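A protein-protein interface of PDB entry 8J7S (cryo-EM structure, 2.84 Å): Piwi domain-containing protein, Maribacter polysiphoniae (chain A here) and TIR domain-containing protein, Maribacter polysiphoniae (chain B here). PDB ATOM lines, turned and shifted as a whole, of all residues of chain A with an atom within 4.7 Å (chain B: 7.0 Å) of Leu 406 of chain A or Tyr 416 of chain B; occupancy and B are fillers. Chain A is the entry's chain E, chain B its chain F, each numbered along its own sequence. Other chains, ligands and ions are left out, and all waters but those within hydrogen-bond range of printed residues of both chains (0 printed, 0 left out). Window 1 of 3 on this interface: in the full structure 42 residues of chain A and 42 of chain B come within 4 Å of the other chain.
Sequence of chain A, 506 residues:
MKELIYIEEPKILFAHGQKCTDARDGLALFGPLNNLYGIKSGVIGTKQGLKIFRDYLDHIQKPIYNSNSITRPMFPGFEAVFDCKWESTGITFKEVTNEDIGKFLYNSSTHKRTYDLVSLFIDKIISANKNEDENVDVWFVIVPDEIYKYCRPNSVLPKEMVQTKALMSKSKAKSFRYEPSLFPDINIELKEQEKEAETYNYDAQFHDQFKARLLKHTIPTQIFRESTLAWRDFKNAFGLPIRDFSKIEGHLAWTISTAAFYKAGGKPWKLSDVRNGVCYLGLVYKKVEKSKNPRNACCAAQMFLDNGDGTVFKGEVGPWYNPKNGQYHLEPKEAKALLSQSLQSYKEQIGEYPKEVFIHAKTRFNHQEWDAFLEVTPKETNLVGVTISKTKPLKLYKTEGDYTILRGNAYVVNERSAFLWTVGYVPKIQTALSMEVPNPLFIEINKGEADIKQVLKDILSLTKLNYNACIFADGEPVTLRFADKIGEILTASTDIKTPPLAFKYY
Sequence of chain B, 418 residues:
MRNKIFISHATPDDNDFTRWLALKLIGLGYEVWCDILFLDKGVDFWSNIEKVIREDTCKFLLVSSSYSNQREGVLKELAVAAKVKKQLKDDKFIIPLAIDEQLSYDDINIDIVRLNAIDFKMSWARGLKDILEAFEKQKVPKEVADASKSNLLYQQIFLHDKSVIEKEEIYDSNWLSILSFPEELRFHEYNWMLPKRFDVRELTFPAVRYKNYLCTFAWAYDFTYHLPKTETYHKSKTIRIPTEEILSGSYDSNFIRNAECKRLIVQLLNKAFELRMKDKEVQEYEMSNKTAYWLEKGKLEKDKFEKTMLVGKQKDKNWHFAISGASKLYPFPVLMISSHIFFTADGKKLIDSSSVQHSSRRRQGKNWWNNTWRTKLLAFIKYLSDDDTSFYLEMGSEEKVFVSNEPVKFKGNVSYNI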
ATOM      1  N   TYR A   6      11.389  23.638 -27.383  1.00  0.00           N
ATOM      2  CA  TYR A   6      10.305  24.194 -28.175  1.00  0.00           C
ATOM      3  C   TYR A   6      10.678  24.151 -29.648  1.00  0.00           C
ATOM      4  O   TYR A   6      11.811  24.468 -30.020  1.00  0.00           O
ATOM      5  CB  TYR A   6       9.995  25.630 -27.763  1.00  0.00           C
ATOM      6  CG  TYR A   6       8.923  26.286 -28.597  1.00  0.00           C
ATOM      7  CD1 TYR A   6       7.581  26.015 -28.374  1.00  0.00           C
ATOM      8  CD2 TYR A   6       9.252  27.182 -29.603  1.00  0.00           C
ATOM      9  CE1 TYR A   6       6.598  26.613 -29.136  1.00  0.00           C
ATOM     10  CE2 TYR A   6       8.276  27.785 -30.368  1.00  0.00           C
ATOM     11  CZ  TYR A   6       6.949  27.496 -30.129  1.00  0.00           C
ATOM     12  OH  TYR A   6       5.969  28.095 -30.886  1.00  0.00           O
ATOM     13  N   LYS A 398      -0.126  21.160 -17.137  1.00  0.00           N
ATOM     14  CA  LYS A 398       0.245  22.533 -16.814  1.00  0.00           C
ATOM     15  C   LYS A 398      -0.239  22.832 -15.402  1.00  0.00           C
ATOM     16  O   LYS A 398      -1.444  22.965 -15.164  1.00  0.00           O
ATOM     17  CB  LYS A 398      -0.344  23.509 -17.827  1.00  0.00           C
ATOM     18  CG  LYS A 398       0.419  24.821 -17.925  1.00  0.00           C
ATOM     19  CD  LYS A 398      -0.201  25.753 -18.951  1.00  0.00           C
ATOM     20  CE  LYS A 398       0.759  26.865 -19.338  1.00  0.00           C
ATOM     21  NZ  LYS A 398       0.404  28.157 -18.691  1.00  0.00           N
ATOM     22  N   TYR A 403      -5.614  25.519 -18.456  1.00  0.00           N
ATOM     23  CA  TYR A 403      -5.283  25.108 -19.811  1.00  0.00           C
ATOM     24  C   TYR A 403      -4.200  24.030 -19.812  1.00  0.00           C
ATOM     25  O   TYR A 403      -3.671  23.635 -18.771  1.00  0.00           O
ATOM     26  CB  TYR A 403      -4.865  26.318 -20.642  1.00  0.00           C
ATOM     27  CG  TYR A 403      -5.905  27.410 -20.666  1.00  0.00           C
ATOM     28  CD1 TYR A 403      -7.257  27.107 -20.590  1.00  0.00           C
ATOM     29  CD2 TYR A 403      -5.539  28.744 -20.764  1.00  0.00           C
ATOM     30  CE1 TYR A 403      -8.215  28.099 -20.610  1.00  0.00           C
ATOM     31  CE2 TYR A 403      -6.490  29.745 -20.786  1.00  0.00           C
ATOM     32  CZ  TYR A 403      -7.827  29.416 -20.709  1.00  0.00           C
ATOM     33  OH  TYR A 403      -8.778  30.408 -20.731  1.00  0.00           O
ATOM     34  N   THR A 404      -3.862  23.553 -21.008  1.00  0.00           N
ATOM     35  CA  THR A 404      -2.979  22.415 -21.189  1.00  0.00           C
ATOM     36  C   THR A 404      -1.593  22.871 -21.638  1.00  0.00           C
ATOM     37  O   THR A 404      -1.292  24.064 -21.722  1.00  0.00           O
ATOM     38  CB  THR A 404      -3.576  21.435 -22.200  1.00  0.00           C
ATOM     39  OG1 THR A 404      -3.217  21.840 -23.525  1.00  0.00           O
ATOM     40  CG2 THR A 404      -5.090  21.410 -22.078  1.00  0.00           C
ATOM     41  N   ILE A 405      -0.736  21.891 -21.931  1.00  0.00           N
ATOM     42  CA  ILE A 405       0.633  22.178 -22.336  1.00  0.00           C
ATOM     43  C   ILE A 405       0.645  22.746 -23.748  1.00  0.00           C
ATOM     44  O   ILE A 405      -0.024  22.231 -24.652  1.00  0.00           O
ATOM     45  CB  ILE A 405       1.498  20.910 -22.235  1.00  0.00           C
ATOM     46  CG1 ILE A 405       2.729  21.023 -23.135  1.00  0.00           C
ATOM     47  CG2 ILE A 405       0.682  19.684 -22.599  1.00  0.00           C
ATOM     48  CD1 ILE A 405       3.692  19.872 -22.994  1.00  0.00           C
ATOM     49  N   LEU A 406       1.407  23.821 -23.936  1.00  0.00           N
ATOM     50  CA  LEU A 406       1.511  24.464 -25.238  1.00  0.00           C
ATOM     51  C   LEU A 406       1.994  23.480 -26.298  1.00  0.00           C
ATOM     52  O   LEU A 406       2.909  22.688 -26.063  1.00  0.00           O
ATOM     53  CB  LEU A 406       2.455  25.663 -25.141  1.00  0.00           C
ATOM     54  CG  LEU A 406       3.046  26.284 -26.403  1.00  0.00           C
ATOM     55  CD1 LEU A 406       3.173  27.781 -26.224  1.00  0.00           C
ATOM     56  CD2 LEU A 406       4.410  25.680 -26.680  1.00  0.00           C
ATOM     57  N   ARG A 407       1.367  23.539 -27.471  1.00  0.00           N
ATOM     58  CA  ARG A 407       1.715  22.640 -28.564  1.00  0.00           C
ATOM     59  C   ARG A 407       3.037  23.054 -29.199  1.00  0.00           C
ATOM     60  O   ARG A 407       3.259  24.234 -29.489  1.00  0.00           O
ATOM     61  CB  ARG A 407       0.608  22.633 -29.613  1.00  0.00           C
ATOM     62  CG  ARG A 407       1.049  22.119 -30.967  1.00  0.00           C
ATOM     63  CD  ARG A 407       0.179  22.668 -32.075  1.00  0.00           C
ATOM     64  NE  ARG A 407       0.027  21.698 -33.151  1.00  0.00           N
ATOM     65  CZ  ARG A 407       0.746  21.694 -34.264  1.00  0.00           C
ATOM     66  NH1 ARG A 407       1.660  22.620 -34.500  1.00  0.00           N
ATOM     67  NH2 ARG A 407       0.545  20.735 -35.160  1.00  0.00           N
ATOM     68  N   GLY A 408       3.905  22.078 -29.432  1.00  0.00           N
ATOM     69  CA  GLY A 408       5.234  22.319 -29.955  1.00  0.00           C
ATOM     70  C   GLY A 408       6.343  21.972 -28.992  1.00  0.00           C
ATOM     71  O   GLY A 408       7.517  22.007 -29.383  1.00  0.00           O
ATOM     72  N   ASN A 409       6.013  21.645 -27.746  1.00  0.00           N
ATOM     73  CA  ASN A 409       7.012  21.215 -26.784  1.00  0.00           C
ATOM     74  C   ASN A 409       7.359  19.750 -27.010  1.00  0.00           C
ATOM     75  O   ASN A 409       6.495  18.924 -27.317  1.00  0.00           O
ATOM     76  CB  ASN A 409       6.506  21.414 -25.357  1.00  0.00           C
ATOM     77  CG  ASN A 409       6.234  22.863 -25.035  1.00  0.00           C
ATOM     78  OD1 ASN A 409       5.226  23.192 -24.415  1.00  0.00           O
ATOM     79  ND2 ASN A 409       7.133  23.741 -25.457  1.00  0.00           N
ATOM     80  N   TRP A 421       4.770  16.999 -29.014  1.00  0.00           N
ATOM     81  CA  TRP A 421       3.399  17.407 -28.721  1.00  0.00           C
ATOM     82  C   TRP A 421       2.835  18.084 -29.966  1.00  0.00           C
ATOM     83  O   TRP A 421       2.967  19.294 -30.153  1.00  0.00           O
ATOM     84  CB  TRP A 421       3.339  18.318 -27.496  1.00  0.00           C
ATOM     85  CG  TRP A 421       3.001  17.565 -26.248  1.00  0.00           C
ATOM     86  CD1 TRP A 421       1.759  17.345 -25.731  1.00  0.00           C
ATOM     87  CD2 TRP A 421       3.920  16.900 -25.377  1.00  0.00           C
ATOM     88  NE1 TRP A 421       1.848  16.597 -24.584  1.00  0.00           N
ATOM     89  CE2 TRP A 421       3.166  16.309 -24.347  1.00  0.00           C
ATOM     90  CE3 TRP A 421       5.309  16.752 -25.365  1.00  0.00           C
ATOM     91  CZ2 TRP A 421       3.753  15.583 -23.320  1.00  0.00           C
ATOM     92  CZ3 TRP A 421       5.889  16.031 -24.344  1.00  0.00           C
ATOM     93  CH2 TRP A 421       5.113  15.456 -23.335  1.00  0.00           C
ATOM     94  N   GLY A 424      -1.982  20.307 -28.666  1.00  0.00           N
ATOM     95  CA  GLY A 424      -1.790  21.090 -27.469  1.00  0.00           C
ATOM     96  C   GLY A 424      -2.529  22.401 -27.556  1.00  0.00           C
ATOM     97  O   GLY A 424      -3.431  22.570 -28.377  1.00  0.00           O
ATOM     98  N   TYR A 425      -2.140  23.331 -26.690  1.00  0.00           N
ATOM     99  CA  TYR A 425      -2.726  24.662 -26.706  1.00  0.00           C
ATOM    100  C   TYR A 425      -2.159  25.474 -27.861  1.00  0.00           C
ATOM    101  O   TYR A 425      -0.960  25.421 -28.151  1.00  0.00           O
ATOM    102  CB  TYR A 425      -2.467  25.379 -25.382  1.00  0.00           C
ATOM    103  CG  TYR A 425      -3.206  26.689 -25.242  1.00  0.00           C
ATOM    104  CD1 TYR A 425      -4.503  26.728 -24.755  1.00  0.00           C
ATOM    105  CD2 TYR A 425      -2.602  27.889 -25.593  1.00  0.00           C
ATOM    106  CE1 TYR A 425      -5.178  27.921 -24.623  1.00  0.00           C
ATOM    107  CE2 TYR A 425      -3.272  29.086 -25.463  1.00  0.00           C
ATOM    108  CZ  TYR A 425      -4.559  29.096 -24.979  1.00  0.00           C
ATOM    109  OH  TYR A 425      -5.230  30.289 -24.849  1.00  0.00           O
ATOM    110  N   ASP B 161      -0.373  40.067 -28.882  1.00  0.00           N
ATOM    111  CA  ASP B 161      -0.544  39.364 -27.610  1.00  0.00           C
ATOM    112  C   ASP B 161      -0.991  37.917 -27.802  1.00  0.00           C
ATOM    113  O   ASP B 161      -1.190  37.192 -26.822  1.00  0.00           O
ATOM    114  CB  ASP B 161      -1.491  40.144 -26.668  1.00  0.00           C
ATOM    115  CG  ASP B 161      -2.981  39.979 -26.992  1.00  0.00           C
ATOM    116  OD1 ASP B 161      -3.468  38.855 -27.242  1.00  0.00           O
ATOM    117  OD2 ASP B 161      -3.694  41.004 -26.947  1.00  0.00           O
ATOM    118  N   SER B 163       0.789  35.202 -28.919  1.00  0.00           N
ATOM    119  CA  SER B 163       2.097  34.667 -29.267  1.00  0.00           C
ATOM    120  C   SER B 163       2.675  33.926 -28.072  1.00  0.00           C
ATOM    121  O   SER B 163       2.285  34.158 -26.924  1.00  0.00           O
ATOM    122  CB  SER B 163       3.051  35.776 -29.723  1.00  0.00           C
ATOM    123  OG  SER B 163       4.241  35.233 -30.266  1.00  0.00           O
ATOM    124  N   VAL B 164       3.613  33.025 -28.364  1.00  0.00           N
ATOM    125  CA  VAL B 164       4.332  32.319 -27.314  1.00  0.00           C
ATOM    126  C   VAL B 164       5.270  33.290 -26.608  1.00  0.00           C
ATOM    127  O   VAL B 164       5.936  34.118 -27.247  1.00  0.00           O
ATOM    128  CB  VAL B 164       5.090  31.114 -27.903  1.00  0.00           C
ATOM    129  CG1 VAL B 164       5.087  31.172 -29.423  1.00  0.00           C
ATOM    130  CG2 VAL B 164       6.515  31.036 -27.371  1.00  0.00           C
ATOM    131  N   ILE B 165       5.309  33.211 -25.281  1.00  0.00           N
ATOM    132  CA  ILE B 165       6.143  34.093 -24.477  1.00  0.00           C
ATOM    133  C   ILE B 165       7.287  33.286 -23.878  1.00  0.00           C
ATOM    134  O   ILE B 165       7.228  32.058 -23.757  1.00  0.00           O
ATOM    135  CB  ILE B 165       5.332  34.811 -23.377  1.00  0.00           C
ATOM    136  CG1 ILE B 165       5.406  34.048 -22.054  1.00  0.00           C
ATOM    137  CG2 ILE B 165       3.884  34.985 -23.810  1.00  0.00           C
ATOM    138  CD1 ILE B 165       4.554  34.647 -20.959  1.00  0.00           C
ATOM    139  N   GLU B 166       8.350  33.995 -23.507  1.00  0.00           N
ATOM    140  CA  GLU B 166       9.556  33.385 -22.948  1.00  0.00           C
ATOM    141  C   GLU B 166       9.485  33.473 -21.429  1.00  0.00           C
ATOM    142  O   GLU B 166       9.829  34.501 -20.840  1.00  0.00           O
ATOM    143  CB  GLU B 166      10.807  34.073 -23.483  1.00  0.00           C
ATOM    144  CG  GLU B 166      11.582  33.256 -24.501  1.00  0.00           C
ATOM    145  CD  GLU B 166      12.334  34.124 -25.488  1.00  0.00           C
ATOM    146  OE1 GLU B 166      12.622  35.292 -25.152  1.00  0.00           O
ATOM    147  OE2 GLU B 166      12.634  33.641 -26.600  1.00  0.00           O
ATOM    148  N   LYS B 167       9.041  32.392 -20.794  1.00  0.00           N
ATOM    149  CA  LYS B 167       9.031  32.321 -19.341  1.00  0.00           C
ATOM    150  C   LYS B 167       9.107  30.861 -18.925  1.00  0.00           C
ATOM    151  O   LYS B 167       8.655  29.972 -19.649  1.00  0.00           O
ATOM    152  CB  LYS B 167       7.789  32.996 -18.746  1.00  0.00           C
ATOM    153  CG  LYS B 167       6.486  32.246 -18.948  1.00  0.00           C
ATOM    154  CD  LYS B 167       5.489  32.616 -17.861  1.00  0.00           C
ATOM    155  CE  LYS B 167       4.142  31.952 -18.084  1.00  0.00           C
ATOM    156  NZ  LYS B 167       4.067  30.612 -17.443  1.00  0.00           N
ATOM    157  N   GLU B 169       8.440  27.363 -17.080  1.00  0.00           N
ATOM    158  CA  GLU B 169       7.271  26.613 -16.653  1.00  0.00           C
ATOM    159  C   GLU B 169       7.712  25.253 -16.140  1.00  0.00           C
ATOM    160  O   GLU B 169       8.664  24.659 -16.653  1.00  0.00           O
ATOM    161  CB  GLU B 169       6.270  26.432 -17.798  1.00  0.00           C
ATOM    162  CG  GLU B 169       5.284  27.568 -17.950  1.00  0.00           C
ATOM    163  CD  GLU B 169       4.028  27.362 -17.132  1.00  0.00           C
ATOM    164  OE1 GLU B 169       3.621  26.195 -16.951  1.00  0.00           O
ATOM    165  OE2 GLU B 169       3.447  28.368 -16.677  1.00  0.00           O
ATOM    166  N   TYR B 171       6.061  21.379 -15.286  1.00  0.00           N
ATOM    167  CA  TYR B 171       4.944  20.530 -15.666  1.00  0.00           C
ATOM    168  C   TYR B 171       4.956  19.273 -14.813  1.00  0.00           C
ATOM    169  O   TYR B 171       6.008  18.648 -14.641  1.00  0.00           O
ATOM    170  CB  TYR B 171       5.014  20.151 -17.148  1.00  0.00           C
ATOM    171  CG  TYR B 171       4.981  21.323 -18.101  1.00  0.00           C
ATOM    172  CD1 TYR B 171       3.776  21.865 -18.525  1.00  0.00           C
ATOM    173  CD2 TYR B 171       6.154  21.877 -18.590  1.00  0.00           C
ATOM    174  CE1 TYR B 171       3.741  22.930 -19.400  1.00  0.00           C
ATOM    175  CE2 TYR B 171       6.130  22.943 -19.466  1.00  0.00           C
ATOM    176  CZ  TYR B 171       4.922  23.465 -19.868  1.00  0.00           C
ATOM    177  OH  TYR B 171       4.893  24.528 -20.740  1.00  0.00           O
ATOM    178  N   VAL B 414       9.128  28.277 -22.464  1.00  0.00           N
ATOM    179  CA  VAL B 414       8.157  28.975 -23.296  1.00  0.00           C
ATOM    180  C   VAL B 414       6.758  28.686 -22.771  1.00  0.00           C
ATOM    181  O   VAL B 414       6.450  27.550 -22.393  1.00  0.00           O
ATOM    182  CB  VAL B 414       8.274  28.554 -24.773  1.00  0.00           C
ATOM    183  CG1 VAL B 414       9.261  29.448 -25.504  1.00  0.00           C
ATOM    184  CG2 VAL B 414       8.691  27.103 -24.863  1.00  0.00           C
ATOM    185  N   SER B 415       5.915  29.711 -22.751  1.00  0.00           N
ATOM    186  CA  SER B 415       4.531  29.559 -22.323  1.00  0.00           C
ATOM    187  C   SER B 415       3.716  30.706 -22.910  1.00  0.00           C
ATOM    188  O   SER B 415       4.170  31.414 -23.816  1.00  0.00           O
ATOM    189  CB  SER B 415       4.425  29.511 -20.797  1.00  0.00           C
ATOM    190  OG  SER B 415       3.147  29.944 -20.367  1.00  0.00           O
ATOM    191  N   TYR B 416       2.506  30.886 -22.390  1.00  0.00           N
ATOM    192  CA  TYR B 416       1.570  31.877 -22.896  1.00  0.00           C
ATOM    193  C   TYR B 416       0.900  32.571 -21.719  1.00  0.00           C
ATOM    194  O   TYR B 416       1.083  32.195 -20.559  1.00  0.00           O
ATOM    195  CB  TYR B 416       0.524  31.234 -23.815  1.00  0.00           C
ATOM    196  CG  TYR B 416      -0.114  29.991 -23.234  1.00  0.00           C
ATOM    197  CD1 TYR B 416       0.498  28.751 -23.357  1.00  0.00           C
ATOM    198  CD2 TYR B 416      -1.325  30.058 -22.561  1.00  0.00           C
ATOM    199  CE1 TYR B 416      -0.075  27.618 -22.828  1.00  0.00           C
ATOM    200  CE2 TYR B 416      -1.909  28.927 -22.031  1.00  0.00           C
ATOM    201  CZ  TYR B 416      -1.278  27.709 -22.167  1.00  0.00           C
ATOM    202  OH  TYR B 416      -1.849  26.574 -21.642  1.00  0.00           O
ATOM    203  N   ASN B 417       0.108  33.597 -22.032  1.00  0.00           N
ATOM    204  CA  ASN B 417      -0.565  34.361 -20.987  1.00  0.00           C
ATOM    205  C   ASN B 417      -1.835  33.662 -20.517  1.00  0.00           C
ATOM    206  O   ASN B 417      -1.953  33.284 -19.348  1.00  0.00           O
ATOM    207  CB  ASN B 417      -0.883  35.771 -21.492  1.00  0.00           C
ATOM    208  CG  ASN B 417       0.211  36.331 -22.376  1.00  0.00           C
ATOM    209  OD1 ASN B 417       0.425  35.859 -23.493  1.00  0.00           O
ATOM    210  ND2 ASN B 417       0.914  37.343 -21.880  1.00  0.00           N
ATOM    211  N   ILE B 418      -2.792  33.470 -21.421  1.00  0.00           N
ATOM    212  CA  ILE B 418      -4.065  32.862 -21.058  1.00  0.00           C
ATOM    213  C   ILE B 418      -4.763  32.298 -22.290  1.00  0.00           C
ATOM    214  O   ILE B 418      -4.382  32.591 -23.423  1.00  0.00           O
ATOM    215  CB  ILE B 418      -4.973  33.873 -20.334  1.00  0.00           C
ATOM    216  CG1 ILE B 418      -5.930  33.146 -19.386  1.00  0.00           C
ATOM    217  CG2 ILE B 418      -5.741  34.722 -21.338  1.00  0.00           C
ATOM    218  CD1 ILE B 418      -5.246  32.146 -18.481  1.00  0.00           C
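The backbone carbonyl oxygen (O) of Ile 418 of chain B lies within hydrogen-bond range of the side-chain hydroxyl (OH) of Tyr 425 of chain A (2.8 Å). O of Thr 404 of chain A lies within hydrogen-bond range of OH of Tyr 416 of chain B (2.6 Å). NZ of Lys 398 of chain A lies within salt-bridge range of OE2 of Glu 169 of chain B, at 3.7 Å.
O of Ser 415 of chain B is in hydrogen-bond range of N of Ile 165 of chain B (2.6 Å). NZ of Lys 167 of chain B is in hydrogen-bond range of OG of Ser 415 of chain B (3.1 Å). N of Tyr 425 of chain A is in hydrogen-bond range of O of Ile 405 of chain A. N of Trp 421 of chain A is in hydrogen-bond range of O of Asn 409 of chain A, 3.1 Å away. The backbone carbonyl oxygen of Leu 406 of chain A lies close to the side-chain amide oxygen of Asn 409 of chain A, 2.9 Å away. NZ of Lys 167 of chain B is in salt-bridge range of OE2 of Glu 169 of chain B, 2.5 Å away.
Tyr 6 of chain A touches Val 164 of chain B (OH to CG1, 3.5 Å). Val 414 of chain B touches Tyr 6 of chain A. Tyr 171 of chain B touches Lys 398 of chain A. OG of Ser 415 of chain B touches NZ of Lys 398 of chain A, at 3.7 Å. CD of Lys 398 of chain A touches OH of Tyr 416 of chain B (3.3 Å). Tyr 403 of chain A touches Tyr 416 of chain B. Tyr 403 of chain A touches Ile 418 of chain B. OD1 of Asn 409 of chain A touches OH of Tyr 171 of chain B, 3.9 Å away. Val 414 of chain B touches Asn 409 of chain A. Tyr 425 of chain A touches Tyr 416 of chain B (CE2 to CD2, 3.6 Å).
Printed residues of chain B within 4 Å of Lys 398 of chain A: Glu 169 (3.6 Å), Tyr 171 (3.98 Å), Ser 415 (3.7 Å) and Tyr 416 (3.3 Å). Leu 406 of chain A touches just one residue of chain B: Tyr 416 (3.9 Å). Asp 161 of chain B touches none of the printed residues of chain A. Lys 167 of chain B touches none of the printed residues of chain A. Of the printed residues of chain A, Tyr 171 of chain B touches Lys 398 and Asn 409. The nearest printed residue of chain A that does not touch Tyr 416 of chain B is Ile 405 of chain A (4.8 Å). The nearest printed residue of chain B that does not touch Tyr 425 of chain A is Asn 417 of chain B (6.5 Å).
Hydrophobic or aromatic side chains of chain A that line the printed part of chain B: Tyr 6, Tyr 403, Leu 406 and Tyr 425. Among the printed residues, Asp or Glu carboxylates within 4 Å of a Lys or Arg side-chain nitrogen of the other chain: Lys 398 of chain A with Glu 169 of chain B.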
